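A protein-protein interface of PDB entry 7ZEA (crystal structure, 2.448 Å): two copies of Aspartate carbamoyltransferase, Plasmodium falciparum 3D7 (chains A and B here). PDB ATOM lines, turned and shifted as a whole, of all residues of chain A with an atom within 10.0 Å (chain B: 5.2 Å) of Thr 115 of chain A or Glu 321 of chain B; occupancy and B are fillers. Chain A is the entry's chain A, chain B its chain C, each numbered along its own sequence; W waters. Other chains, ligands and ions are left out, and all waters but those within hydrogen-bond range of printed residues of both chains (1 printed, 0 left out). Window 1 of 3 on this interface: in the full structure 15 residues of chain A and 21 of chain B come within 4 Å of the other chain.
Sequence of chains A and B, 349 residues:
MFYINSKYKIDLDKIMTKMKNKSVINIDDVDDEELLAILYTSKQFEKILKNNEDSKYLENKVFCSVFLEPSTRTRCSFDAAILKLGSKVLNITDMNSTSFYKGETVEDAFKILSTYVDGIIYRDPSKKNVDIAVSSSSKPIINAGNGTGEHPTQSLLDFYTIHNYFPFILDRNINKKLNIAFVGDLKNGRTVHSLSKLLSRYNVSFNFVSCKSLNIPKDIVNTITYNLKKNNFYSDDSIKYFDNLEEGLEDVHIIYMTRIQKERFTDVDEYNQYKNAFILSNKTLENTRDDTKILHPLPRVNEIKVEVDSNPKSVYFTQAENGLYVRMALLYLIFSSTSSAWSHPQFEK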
ATOM      1  N   VAL A  62     -15.469  -6.884 -18.666  1.00  0.00           N
ATOM      2  CA  VAL A  62     -16.035  -5.505 -18.581  1.00  0.00           C
ATOM      3  C   VAL A  62     -15.534  -4.801 -19.817  1.00  0.00           C
ATOM      4  O   VAL A  62     -14.327  -4.841 -20.034  1.00  0.00           O
ATOM      5  CB  VAL A  62     -15.550  -4.783 -17.315  1.00  0.00           C
ATOM      6  CG1 VAL A  62     -16.050  -3.357 -17.268  1.00  0.00           C
ATOM      7  CG2 VAL A  62     -15.892  -5.579 -16.062  1.00  0.00           C
ATOM      8  N   CYS A  64     -15.902  -1.492 -22.780  1.00  0.00           N
ATOM      9  CA  CYS A  64     -16.312  -0.082 -23.013  1.00  0.00           C
ATOM     10  C   CYS A  64     -16.794  -0.009 -24.462  1.00  0.00           C
ATOM     11  O   CYS A  64     -16.137  -0.577 -25.359  1.00  0.00           O
ATOM     12  CB  CYS A  64     -15.214   0.926 -22.730  1.00  0.00           C
ATOM     13  SG  CYS A  64     -15.752   2.605 -23.054  1.00  0.00           S
ATOM     14  N   LEU A  90     -19.764  -0.464 -20.070  1.00  0.00           N
ATOM     15  CA  LEU A  90     -19.729   0.953 -19.727  1.00  0.00           C
ATOM     16  C   LEU A  90     -19.805   1.639 -21.101  1.00  0.00           C
ATOM     17  O   LEU A  90     -19.093   1.193 -22.019  1.00  0.00           O
ATOM     18  CB  LEU A  90     -18.426   0.873 -18.910  1.00  0.00           C
ATOM     19  CG  LEU A  90     -17.464   2.007 -18.769  1.00  0.00           C
ATOM     20  CD1 LEU A  90     -16.140   1.371 -18.433  1.00  0.00           C
ATOM     21  CD2 LEU A  90     -17.357   2.874 -19.996  1.00  0.00           C
ATOM     22  N   GLU A 107      -4.686   9.084 -29.041  1.00  0.00           N
ATOM     23  CA  GLU A 107      -3.666   8.117 -28.542  1.00  0.00           C
ATOM     24  C   GLU A 107      -3.693   8.152 -27.006  1.00  0.00           C
ATOM     25  O   GLU A 107      -3.777   7.047 -26.407  1.00  0.00           O
ATOM     26  CB  GLU A 107      -2.285   8.296 -29.191  1.00  0.00           C
ATOM     27  CG  GLU A 107      -2.037   9.640 -29.865  1.00  0.00           C
ATOM     28  CD  GLU A 107      -2.445   9.886 -31.316  1.00  0.00           C
ATOM     29  OE1 GLU A 107      -1.738   9.374 -32.232  1.00  0.00           O
ATOM     30  OE2 GLU A 107      -3.415  10.699 -31.525  1.00  0.00           O
ATOM     31  N   ASP A 108      -3.734   9.343 -26.389  1.00  0.00           N
ATOM     32  CA  ASP A 108      -3.817   9.462 -24.912  1.00  0.00           C
ATOM     33  C   ASP A 108      -5.130   8.832 -24.455  1.00  0.00           C
ATOM     34  O   ASP A 108      -5.118   8.087 -23.478  1.00  0.00           O
ATOM     35  CB  ASP A 108      -3.704  10.908 -24.410  1.00  0.00           C
ATOM     36  CG  ASP A 108      -2.338  11.580 -24.589  1.00  0.00           C
ATOM     37  OD1 ASP A 108      -1.410  10.870 -25.009  1.00  0.00           O
ATOM     38  OD2 ASP A 108      -2.228  12.834 -24.347  1.00  0.00           O
ATOM     39  N   ALA A 109      -6.232   9.103 -25.143  1.00  0.00           N
ATOM     40  CA  ALA A 109      -7.567   8.690 -24.653  1.00  0.00           C
ATOM     41  C   ALA A 109      -7.640   7.157 -24.647  1.00  0.00           C
ATOM     42  O   ALA A 109      -8.170   6.593 -23.674  1.00  0.00           O
ATOM     43  CB  ALA A 109      -8.686   9.321 -25.455  1.00  0.00           C
ATOM     44  N   PHE A 110      -7.104   6.495 -25.663  1.00  0.00           N
ATOM     45  CA  PHE A 110      -7.214   5.024 -25.784  1.00  0.00           C
ATOM     46  C   PHE A 110      -6.133   4.369 -24.954  1.00  0.00           C
ATOM     47  O   PHE A 110      -6.349   3.257 -24.496  1.00  0.00           O
ATOM     48  CB  PHE A 110      -7.200   4.558 -27.242  1.00  0.00           C
ATOM     49  CG  PHE A 110      -8.591   4.462 -27.794  1.00  0.00           C
ATOM     50  CD1 PHE A 110      -9.247   5.599 -28.229  1.00  0.00           C
ATOM     51  CD2 PHE A 110      -9.291   3.288 -27.721  1.00  0.00           C
ATOM     52  CE1 PHE A 110     -10.557   5.556 -28.661  1.00  0.00           C
ATOM     53  CE2 PHE A 110     -10.595   3.235 -28.180  1.00  0.00           C
ATOM     54  CZ  PHE A 110     -11.221   4.362 -28.645  1.00  0.00           C
ATOM     55  N   LYS A 111      -5.018   5.036 -24.751  1.00  0.00           N
ATOM     56  CA  LYS A 111      -3.954   4.479 -23.875  1.00  0.00           C
ATOM     57  C   LYS A 111      -4.566   4.355 -22.480  1.00  0.00           C
ATOM     58  O   LYS A 111      -4.431   3.291 -21.866  1.00  0.00           O
ATOM     59  CB  LYS A 111      -2.700   5.358 -23.985  1.00  0.00           C
ATOM     60  CG  LYS A 111      -1.483   4.904 -23.186  1.00  0.00           C
ATOM     61  CD  LYS A 111      -0.158   5.428 -23.766  1.00  0.00           C
ATOM     62  CE  LYS A 111       1.057   4.865 -23.046  1.00  0.00           C
ATOM     63  NZ  LYS A 111       1.038   3.373 -22.966  1.00  0.00           N
ATOM     64  N   ILE A 112      -5.282   5.383 -22.043  1.00  0.00           N
ATOM     65  CA  ILE A 112      -5.885   5.431 -20.683  1.00  0.00           C
ATOM     66  C   ILE A 112      -7.087   4.478 -20.596  1.00  0.00           C
ATOM     67  O   ILE A 112      -7.173   3.686 -19.668  1.00  0.00           O
ATOM     68  CB  ILE A 112      -6.298   6.868 -20.316  1.00  0.00           C
ATOM     69  CG1 ILE A 112      -5.087   7.792 -20.232  1.00  0.00           C
ATOM     70  CG2 ILE A 112      -7.073   6.871 -19.001  1.00  0.00           C
ATOM     71  CD1 ILE A 112      -5.426   9.244 -20.480  1.00  0.00           C
ATOM     72  N   LEU A 113      -8.035   4.630 -21.492  1.00  0.00           N
ATOM     73  CA  LEU A 113      -9.304   3.892 -21.427  1.00  0.00           C
ATOM     74  C   LEU A 113      -9.022   2.388 -21.482  1.00  0.00           C
ATOM     75  O   LEU A 113      -9.755   1.641 -20.772  1.00  0.00           O
ATOM     76  CB  LEU A 113     -10.178   4.367 -22.582  1.00  0.00           C
ATOM     77  CG  LEU A 113     -11.505   3.657 -22.702  1.00  0.00           C
ATOM     78  CD1 LEU A 113     -12.320   3.927 -21.433  1.00  0.00           C
ATOM     79  CD2 LEU A 113     -12.212   4.124 -23.960  1.00  0.00           C
ATOM     80  N   SER A 114      -7.991   1.948 -22.211  1.00  0.00           N
ATOM     81  CA  SER A 114      -7.676   0.509 -22.324  1.00  0.00           C
ATOM     82  C   SER A 114      -7.159  -0.038 -20.994  1.00  0.00           C
ATOM     83  O   SER A 114      -7.189  -1.262 -20.842  1.00  0.00           O
ATOM     84  CB  SER A 114      -6.723   0.173 -23.459  1.00  0.00           C
ATOM     85  OG  SER A 114      -5.543   0.945 -23.482  1.00  0.00           O
ATOM     86  N   THR A 115      -6.748   0.799 -20.044  1.00  0.00           N
ATOM     87  CA  THR A 115      -6.311   0.320 -18.712  1.00  0.00           C
ATOM     88  C   THR A 115      -7.538  -0.035 -17.858  1.00  0.00           C
ATOM     89  O   THR A 115      -7.354  -0.781 -16.908  1.00  0.00           O
ATOM     90  CB  THR A 115      -5.407   1.354 -18.028  1.00  0.00           C
ATOM     91  OG1 THR A 115      -6.142   2.499 -17.592  1.00  0.00           O
ATOM     92  CG2 THR A 115      -4.286   1.809 -18.940  1.00  0.00           C
ATOM     93  N   TYR A 116      -8.736   0.469 -18.183  1.00  0.00           N
ATOM     94  CA  TYR A 116      -9.976   0.350 -17.359  1.00  0.00           C
ATOM     95  C   TYR A 116     -10.738  -0.931 -17.686  1.00  0.00           C
ATOM     96  O   TYR A 116     -11.458  -1.441 -16.820  1.00  0.00           O
ATOM     97  CB  TYR A 116     -10.954   1.507 -17.629  1.00  0.00           C
ATOM     98  CG  TYR A 116     -10.484   2.893 -17.254  1.00  0.00           C
ATOM     99  CD1 TYR A 116      -9.348   3.082 -16.489  1.00  0.00           C
ATOM    100  CD2 TYR A 116     -11.212   4.017 -17.621  1.00  0.00           C
ATOM    101  CE1 TYR A 116      -8.926   4.351 -16.098  1.00  0.00           C
ATOM    102  CE2 TYR A 116     -10.778   5.295 -17.292  1.00  0.00           C
ATOM    103  CZ  TYR A 116      -9.646   5.470 -16.494  1.00  0.00           C
ATOM    104  OH  TYR A 116      -9.203   6.706 -16.066  1.00  0.00           O
ATOM    105  N   VAL A 117     -10.613  -1.436 -18.918  1.00  0.00           N
ATOM    106  CA  VAL A 117     -11.550  -2.473 -19.463  1.00  0.00           C
ATOM    107  C   VAL A 117     -10.790  -3.604 -20.133  1.00  0.00           C
ATOM    108  O   VAL A 117      -9.599  -3.404 -20.413  1.00  0.00           O
ATOM    109  CB  VAL A 117     -12.555  -1.839 -20.427  1.00  0.00           C
ATOM    110  CG1 VAL A 117     -13.442  -0.859 -19.683  1.00  0.00           C
ATOM    111  CG2 VAL A 117     -11.858  -1.162 -21.600  1.00  0.00           C
ATOM    112  N   ASP A 118     -11.487  -4.714 -20.413  1.00  0.00           N
ATOM    113  CA  ASP A 118     -10.919  -5.902 -21.102  1.00  0.00           C
ATOM    114  C   ASP A 118     -10.920  -5.756 -22.627  1.00  0.00           C
ATOM    115  O   ASP A 118     -10.098  -6.436 -23.274  1.00  0.00           O
ATOM    116  CB  ASP A 118     -11.660  -7.157 -20.715  1.00  0.00           C
ATOM    117  CG  ASP A 118     -11.592  -7.380 -19.231  1.00  0.00           C
ATOM    118  OD1 ASP A 118     -10.480  -7.499 -18.734  1.00  0.00           O
ATOM    119  OD2 ASP A 118     -12.673  -7.412 -18.601  1.00  0.00           O
ATOM    120  N   GLY A 119     -11.726  -4.855 -23.166  1.00  0.00           N
ATOM    121  CA  GLY A 119     -11.816  -4.611 -24.602  1.00  0.00           C
ATOM    122  C   GLY A 119     -12.763  -3.465 -24.924  1.00  0.00           C
ATOM    123  O   GLY A 119     -13.513  -3.023 -24.064  1.00  0.00           O
ATOM    124  N   ILE A 120     -12.696  -2.961 -26.141  1.00  0.00           N
ATOM    125  CA  ILE A 120     -13.415  -1.738 -26.544  1.00  0.00           C
ATOM    126  C   ILE A 120     -14.121  -2.012 -27.865  1.00  0.00           C
ATOM    127  O   ILE A 120     -13.480  -2.515 -28.782  1.00  0.00           O
ATOM    128  CB  ILE A 120     -12.450  -0.564 -26.674  1.00  0.00           C
ATOM    129  CG1 ILE A 120     -11.794  -0.294 -25.331  1.00  0.00           C
ATOM    130  CG2 ILE A 120     -13.168   0.652 -27.226  1.00  0.00           C
ATOM    131  CD1 ILE A 120     -10.698   0.704 -25.365  1.00  0.00           C
ATOM    132  N   SER A 136      -2.719   2.547 -29.975  1.00  0.00           N
ATOM    133  CA  SER A 136      -2.568   3.106 -28.602  1.00  0.00           C
ATOM    134  C   SER A 136      -3.122   2.153 -27.548  1.00  0.00           C
ATOM    135  O   SER A 136      -2.646   2.241 -26.388  1.00  0.00           O
ATOM    136  CB  SER A 136      -3.249   4.423 -28.468  1.00  0.00           C
ATOM    137  OG  SER A 136      -2.993   5.239 -29.599  1.00  0.00           O
ATOM    138  N   SER A 137      -4.115   1.336 -27.912  1.00  0.00           N
ATOM    139  CA  SER A 137      -4.880   0.502 -26.964  1.00  0.00           C
ATOM    140  C   SER A 137      -4.032  -0.681 -26.516  1.00  0.00           C
ATOM    141  O   SER A 137      -3.604  -1.371 -27.364  1.00  0.00           O
ATOM    142  CB  SER A 137      -6.177   0.018 -27.566  1.00  0.00           C
ATOM    143  OG  SER A 137      -6.830  -0.868 -26.660  1.00  0.00           O
ATOM    144  N   SER A 138      -3.936  -0.957 -25.213  1.00  0.00           N
ATOM    145  CA  SER A 138      -3.398  -2.235 -24.662  1.00  0.00           C
ATOM    146  C   SER A 138      -4.453  -3.349 -24.762  1.00  0.00           C
ATOM    147  O   SER A 138      -4.173  -4.435 -24.296  1.00  0.00           O
ATOM    148  CB  SER A 138      -2.915  -2.063 -23.224  1.00  0.00           C
ATOM    149  OG  SER A 138      -3.981  -1.664 -22.356  1.00  0.00           O
ATOM    150  N   LYS A 139      -5.634  -3.094 -25.326  1.00  0.00           N
ATOM    151  CA  LYS A 139      -6.727  -4.083 -25.342  1.00  0.00           C
ATOM    152  C   LYS A 139      -7.329  -4.203 -26.735  1.00  0.00           C
ATOM    153  O   LYS A 139      -7.313  -3.273 -27.529  1.00  0.00           O
ATOM    154  CB  LYS A 139      -7.799  -3.706 -24.327  1.00  0.00           C
ATOM    155  CG  LYS A 139      -7.309  -3.705 -22.880  1.00  0.00           C
ATOM    156  CD  LYS A 139      -6.889  -5.066 -22.324  1.00  0.00           C
ATOM    157  CE  LYS A 139      -6.080  -4.962 -21.060  1.00  0.00           C
ATOM    158  NZ  LYS A 139      -6.708  -4.034 -20.092  1.00  0.00           N
ATOM    159  N   PRO A 140      -7.916  -5.377 -27.051  1.00  0.00           N
ATOM    160  CA  PRO A 140      -8.544  -5.589 -28.345  1.00  0.00           C
ATOM    161  C   PRO A 140      -9.633  -4.573 -28.645  1.00  0.00           C
ATOM    162  O   PRO A 140     -10.434  -4.271 -27.803  1.00  0.00           O
ATOM    163  CB  PRO A 140      -9.124  -6.980 -28.212  1.00  0.00           C
ATOM    164  CG  PRO A 140      -8.192  -7.633 -27.198  1.00  0.00           C
ATOM    165  CD  PRO A 140      -7.990  -6.546 -26.169  1.00  0.00           C
ATOM    166  N   LYS B  50      -3.836  -7.572 -12.737  1.00  0.00           N
ATOM    167  CA  LYS B  50      -2.658  -7.830 -13.603  1.00  0.00           C
ATOM    168  C   LYS B  50      -2.474  -9.350 -13.773  1.00  0.00           C
ATOM    169  O   LYS B  50      -2.009  -9.733 -14.834  1.00  0.00           O
ATOM    170  CB  LYS B  50      -1.413  -7.144 -13.060  1.00  0.00           C
ATOM    171  CG  LYS B  50      -1.404  -5.622 -13.230  1.00  0.00           C
ATOM    172  CD  LYS B  50      -0.084  -4.995 -12.754  1.00  0.00           C
ATOM    173  CE  LYS B  50       0.071  -3.534 -13.122  1.00  0.00           C
ATOM    174  NZ  LYS B  50       1.435  -3.013 -12.818  1.00  0.00           N
ATOM    175  N   PHE B 317       0.615   7.684 -17.194  1.00  0.00           N
ATOM    176  CA  PHE B 317      -0.377   6.708 -17.722  1.00  0.00           C
ATOM    177  C   PHE B 317      -0.558   5.596 -16.687  1.00  0.00           C
ATOM    178  O   PHE B 317      -1.715   5.208 -16.468  1.00  0.00           O
ATOM    179  CB  PHE B 317      -0.006   6.221 -19.121  1.00  0.00           C
ATOM    180  CG  PHE B 317      -0.163   7.273 -20.185  1.00  0.00           C
ATOM    181  CD1 PHE B 317      -1.398   7.792 -20.499  1.00  0.00           C
ATOM    182  CD2 PHE B 317       0.937   7.746 -20.879  1.00  0.00           C
ATOM    183  CE1 PHE B 317      -1.536   8.748 -21.500  1.00  0.00           C
ATOM    184  CE2 PHE B 317       0.811   8.720 -21.863  1.00  0.00           C
ATOM    185  CZ  PHE B 317      -0.431   9.218 -22.176  1.00  0.00           C
ATOM    186  N   THR B 318       0.500   5.159 -16.000  1.00  0.00           N
ATOM    187  CA  THR B 318       0.331   4.196 -14.882  1.00  0.00           C
ATOM    188  C   THR B 318      -0.540   4.837 -13.788  1.00  0.00           C
ATOM    189  O   THR B 318      -1.377   4.128 -13.192  1.00  0.00           O
ATOM    190  CB  THR B 318       1.671   3.699 -14.342  1.00  0.00           C
ATOM    191  OG1 THR B 318       2.398   3.202 -15.452  1.00  0.00           O
ATOM    192  CG2 THR B 318       1.559   2.612 -13.286  1.00  0.00           C
ATOM    193  N   GLN B 319      -0.330   6.137 -13.535  1.00  0.00           N
ATOM    194  CA  GLN B 319      -1.088   6.966 -12.561  1.00  0.00           C
ATOM    195  C   GLN B 319      -2.599   6.839 -12.836  1.00  0.00           C
ATOM    196  O   GLN B 319      -3.316   6.388 -11.955  1.00  0.00           O
ATOM    197  CB  GLN B 319      -0.582   8.404 -12.681  1.00  0.00           C
ATOM    198  CG  GLN B 319      -1.204   9.392 -11.721  1.00  0.00           C
ATOM    199  CD  GLN B 319      -0.807  10.810 -12.033  1.00  0.00           C
ATOM    200  OE1 GLN B 319       0.032  11.081 -12.889  1.00  0.00           O
ATOM    201  NE2 GLN B 319      -1.396  11.735 -11.293  1.00  0.00           N
ATOM    202  N   ALA B 320      -3.039   7.205 -14.029  1.00  0.00           N
ATOM    203  CA  ALA B 320      -4.438   7.127 -14.488  1.00  0.00           C
ATOM    204  C   ALA B 320      -4.957   5.686 -14.332  1.00  0.00           C
ATOM    205  O   ALA B 320      -6.056   5.476 -13.795  1.00  0.00           O
ATOM    206  CB  ALA B 320      -4.510   7.598 -15.904  1.00  0.00           C
ATOM    207  N   GLU B 321      -4.180   4.708 -14.749  1.00  0.00           N
ATOM    208  CA  GLU B 321      -4.498   3.280 -14.545  1.00  0.00           C
ATOM    209  C   GLU B 321      -4.761   3.042 -13.051  1.00  0.00           C
ATOM    210  O   GLU B 321      -5.756   2.390 -12.730  1.00  0.00           O
ATOM    211  CB  GLU B 321      -3.375   2.428 -15.134  1.00  0.00           C
ATOM    212  CG  GLU B 321      -3.512   0.939 -14.900  1.00  0.00           C
ATOM    213  CD  GLU B 321      -2.227   0.200 -15.246  1.00  0.00           C
ATOM    214  OE1 GLU B 321      -1.411   0.760 -16.022  1.00  0.00           O
ATOM    215  OE2 GLU B 321      -1.969  -0.862 -14.670  1.00  0.00           O
ATOM    216  N   ASN B 322      -3.916   3.539 -12.155  1.00  0.00           N
ATOM    217  CA  ASN B 322      -4.024   3.243 -10.699  1.00  0.00           C
ATOM    218  C   ASN B 322      -5.362   3.741 -10.141  1.00  0.00           C
ATOM    219  O   ASN B 322      -5.801   3.208  -9.111  1.00  0.00           O
ATOM    220  CB  ASN B 322      -2.899   3.867  -9.910  1.00  0.00           C
ATOM    221  CG  ASN B 322      -1.562   3.221 -10.162  1.00  0.00           C
ATOM    222  OD1 ASN B 322      -1.471   2.035 -10.517  1.00  0.00           O
ATOM    223  ND2 ASN B 322      -0.508   3.996  -9.931  1.00  0.00           N
ATOM    224  N   GLY B 323      -5.975   4.720 -10.805  1.00  0.00           N
ATOM    225  CA  GLY B 323      -7.336   5.207 -10.493  1.00  0.00           C
ATOM    226  C   GLY B 323      -8.328   4.065 -10.414  1.00  0.00           C
ATOM    227  O   GLY B 323      -9.161   4.095  -9.547  1.00  0.00           O
ATOM    228  N   LEU B 324      -8.219   3.069 -11.299  1.00  0.00           N
ATOM    229  CA  LEU B 324      -9.135   1.915 -11.302  1.00  0.00           C
ATOM    230  C   LEU B 324      -8.958   1.213  -9.962  1.00  0.00           C
ATOM    231  O   LEU B 324      -9.959   0.912  -9.322  1.00  0.00           O
ATOM    232  CB  LEU B 324      -8.845   0.987 -12.490  1.00  0.00           C
ATOM    233  CG  LEU B 324      -9.591  -0.349 -12.478  1.00  0.00           C
ATOM    234  CD1 LEU B 324     -11.105  -0.125 -12.498  1.00  0.00           C
ATOM    235  CD2 LEU B 324      -9.144  -1.244 -13.651  1.00  0.00           C
ATOM    236  N   TYR B 325      -7.730   0.929  -9.555  1.00  0.00           N
ATOM    237  CA  TYR B 325      -7.480   0.066  -8.369  1.00  0.00           C
ATOM    238  C   TYR B 325      -7.850   0.846  -7.102  1.00  0.00           C
ATOM    239  O   TYR B 325      -8.366   0.256  -6.167  1.00  0.00           O
ATOM    240  CB  TYR B 325      -6.025  -0.358  -8.312  1.00  0.00           C
ATOM    241  CG  TYR B 325      -5.468  -0.844  -9.626  1.00  0.00           C
ATOM    242  CD1 TYR B 325      -6.120  -1.809 -10.374  1.00  0.00           C
ATOM    243  CD2 TYR B 325      -4.265  -0.372 -10.102  1.00  0.00           C
ATOM    244  CE1 TYR B 325      -5.591  -2.296 -11.559  1.00  0.00           C
ATOM    245  CE2 TYR B 325      -3.728  -0.824 -11.287  1.00  0.00           C
ATOM    246  CZ  TYR B 325      -4.395  -1.788 -12.021  1.00  0.00           C
ATOM    247  OH  TYR B 325      -3.835  -2.208 -13.182  1.00  0.00           O
HETATM  248  O   HOH W   1      -8.006   7.286 -13.394  1.00  0.00           O
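O of Ile 112 of chain A sits at hydrogen-bond distance from OG1 of Thr 115 of chain A. The side-chain carboxylate of Glu 321 of chain B sits at hydrogen-bond distance from the side-chain hydroxyl of Tyr 325 of chain B (2.7 Å). The side-chain hydroxyl (OG) of Ser 114 of chain A sits at hydrogen-bond distance from the backbone carbonyl oxygen (O) of Lys 111 of chain A, at 3.1 Å.
Among the printed residues, pairs that only touch across the chains: Asp 108 of chain A with Phe 317 of chain B, Lys 111 of chain A with Phe 317 of chain B, Ile 112 of chain A with Phe 317 of chain B, Thr 115 of chain A with Glu 321 of chain B, Thr 115 of chain A with Leu 324 of chain B, Tyr 116 of chain A with Ala 320 of chain B and Tyr 116 of chain A with Leu 324 of chain B.
Printed residues of chain B within 4 Å of Asp 108 of chain A: Phe 317 (3.4 Å). Of the printed residues of chain B, Lys 111 of chain A touches Phe 317 (3.6 Å). Of the printed residues of chain B, Thr 115 of chain A touches Glu 321 and Leu 324. Printed residues of chain B within 4 Å of Tyr 116 of chain A: Ala 320 and Leu 324. Of the printed residues of chain A, Phe 317 of chain B touches Asp 108 (3.4 Å), Lys 111 (3.6 Å) and Ile 112 (3.7 Å). Thr 318 of chain B touches none of the printed residues of chain A. Glu 321 of chain B touches one residue of chain A.
Hydrophobic or aromatic side chains of chain B that line the printed part of chain A: Phe 317 and Leu 324. Of the 22 printed residues of chain A, 5 touch a printed residue of chain B. Hydrophobic or aromatic side chains of chain A that line the printed part of chain B: Ile 112 and Tyr 116. Among the printed residues, 7 pairs touch across the chains.
No position is printed for both chains. Of the 7 pairs that touch across the chains among the printed residues, none has its exchanged pair printed and touching as well.
Water W1 bridges O of Ala 320 of chain B (2.7 Å) and OH of Tyr 116 of chain A (3.0 Å).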
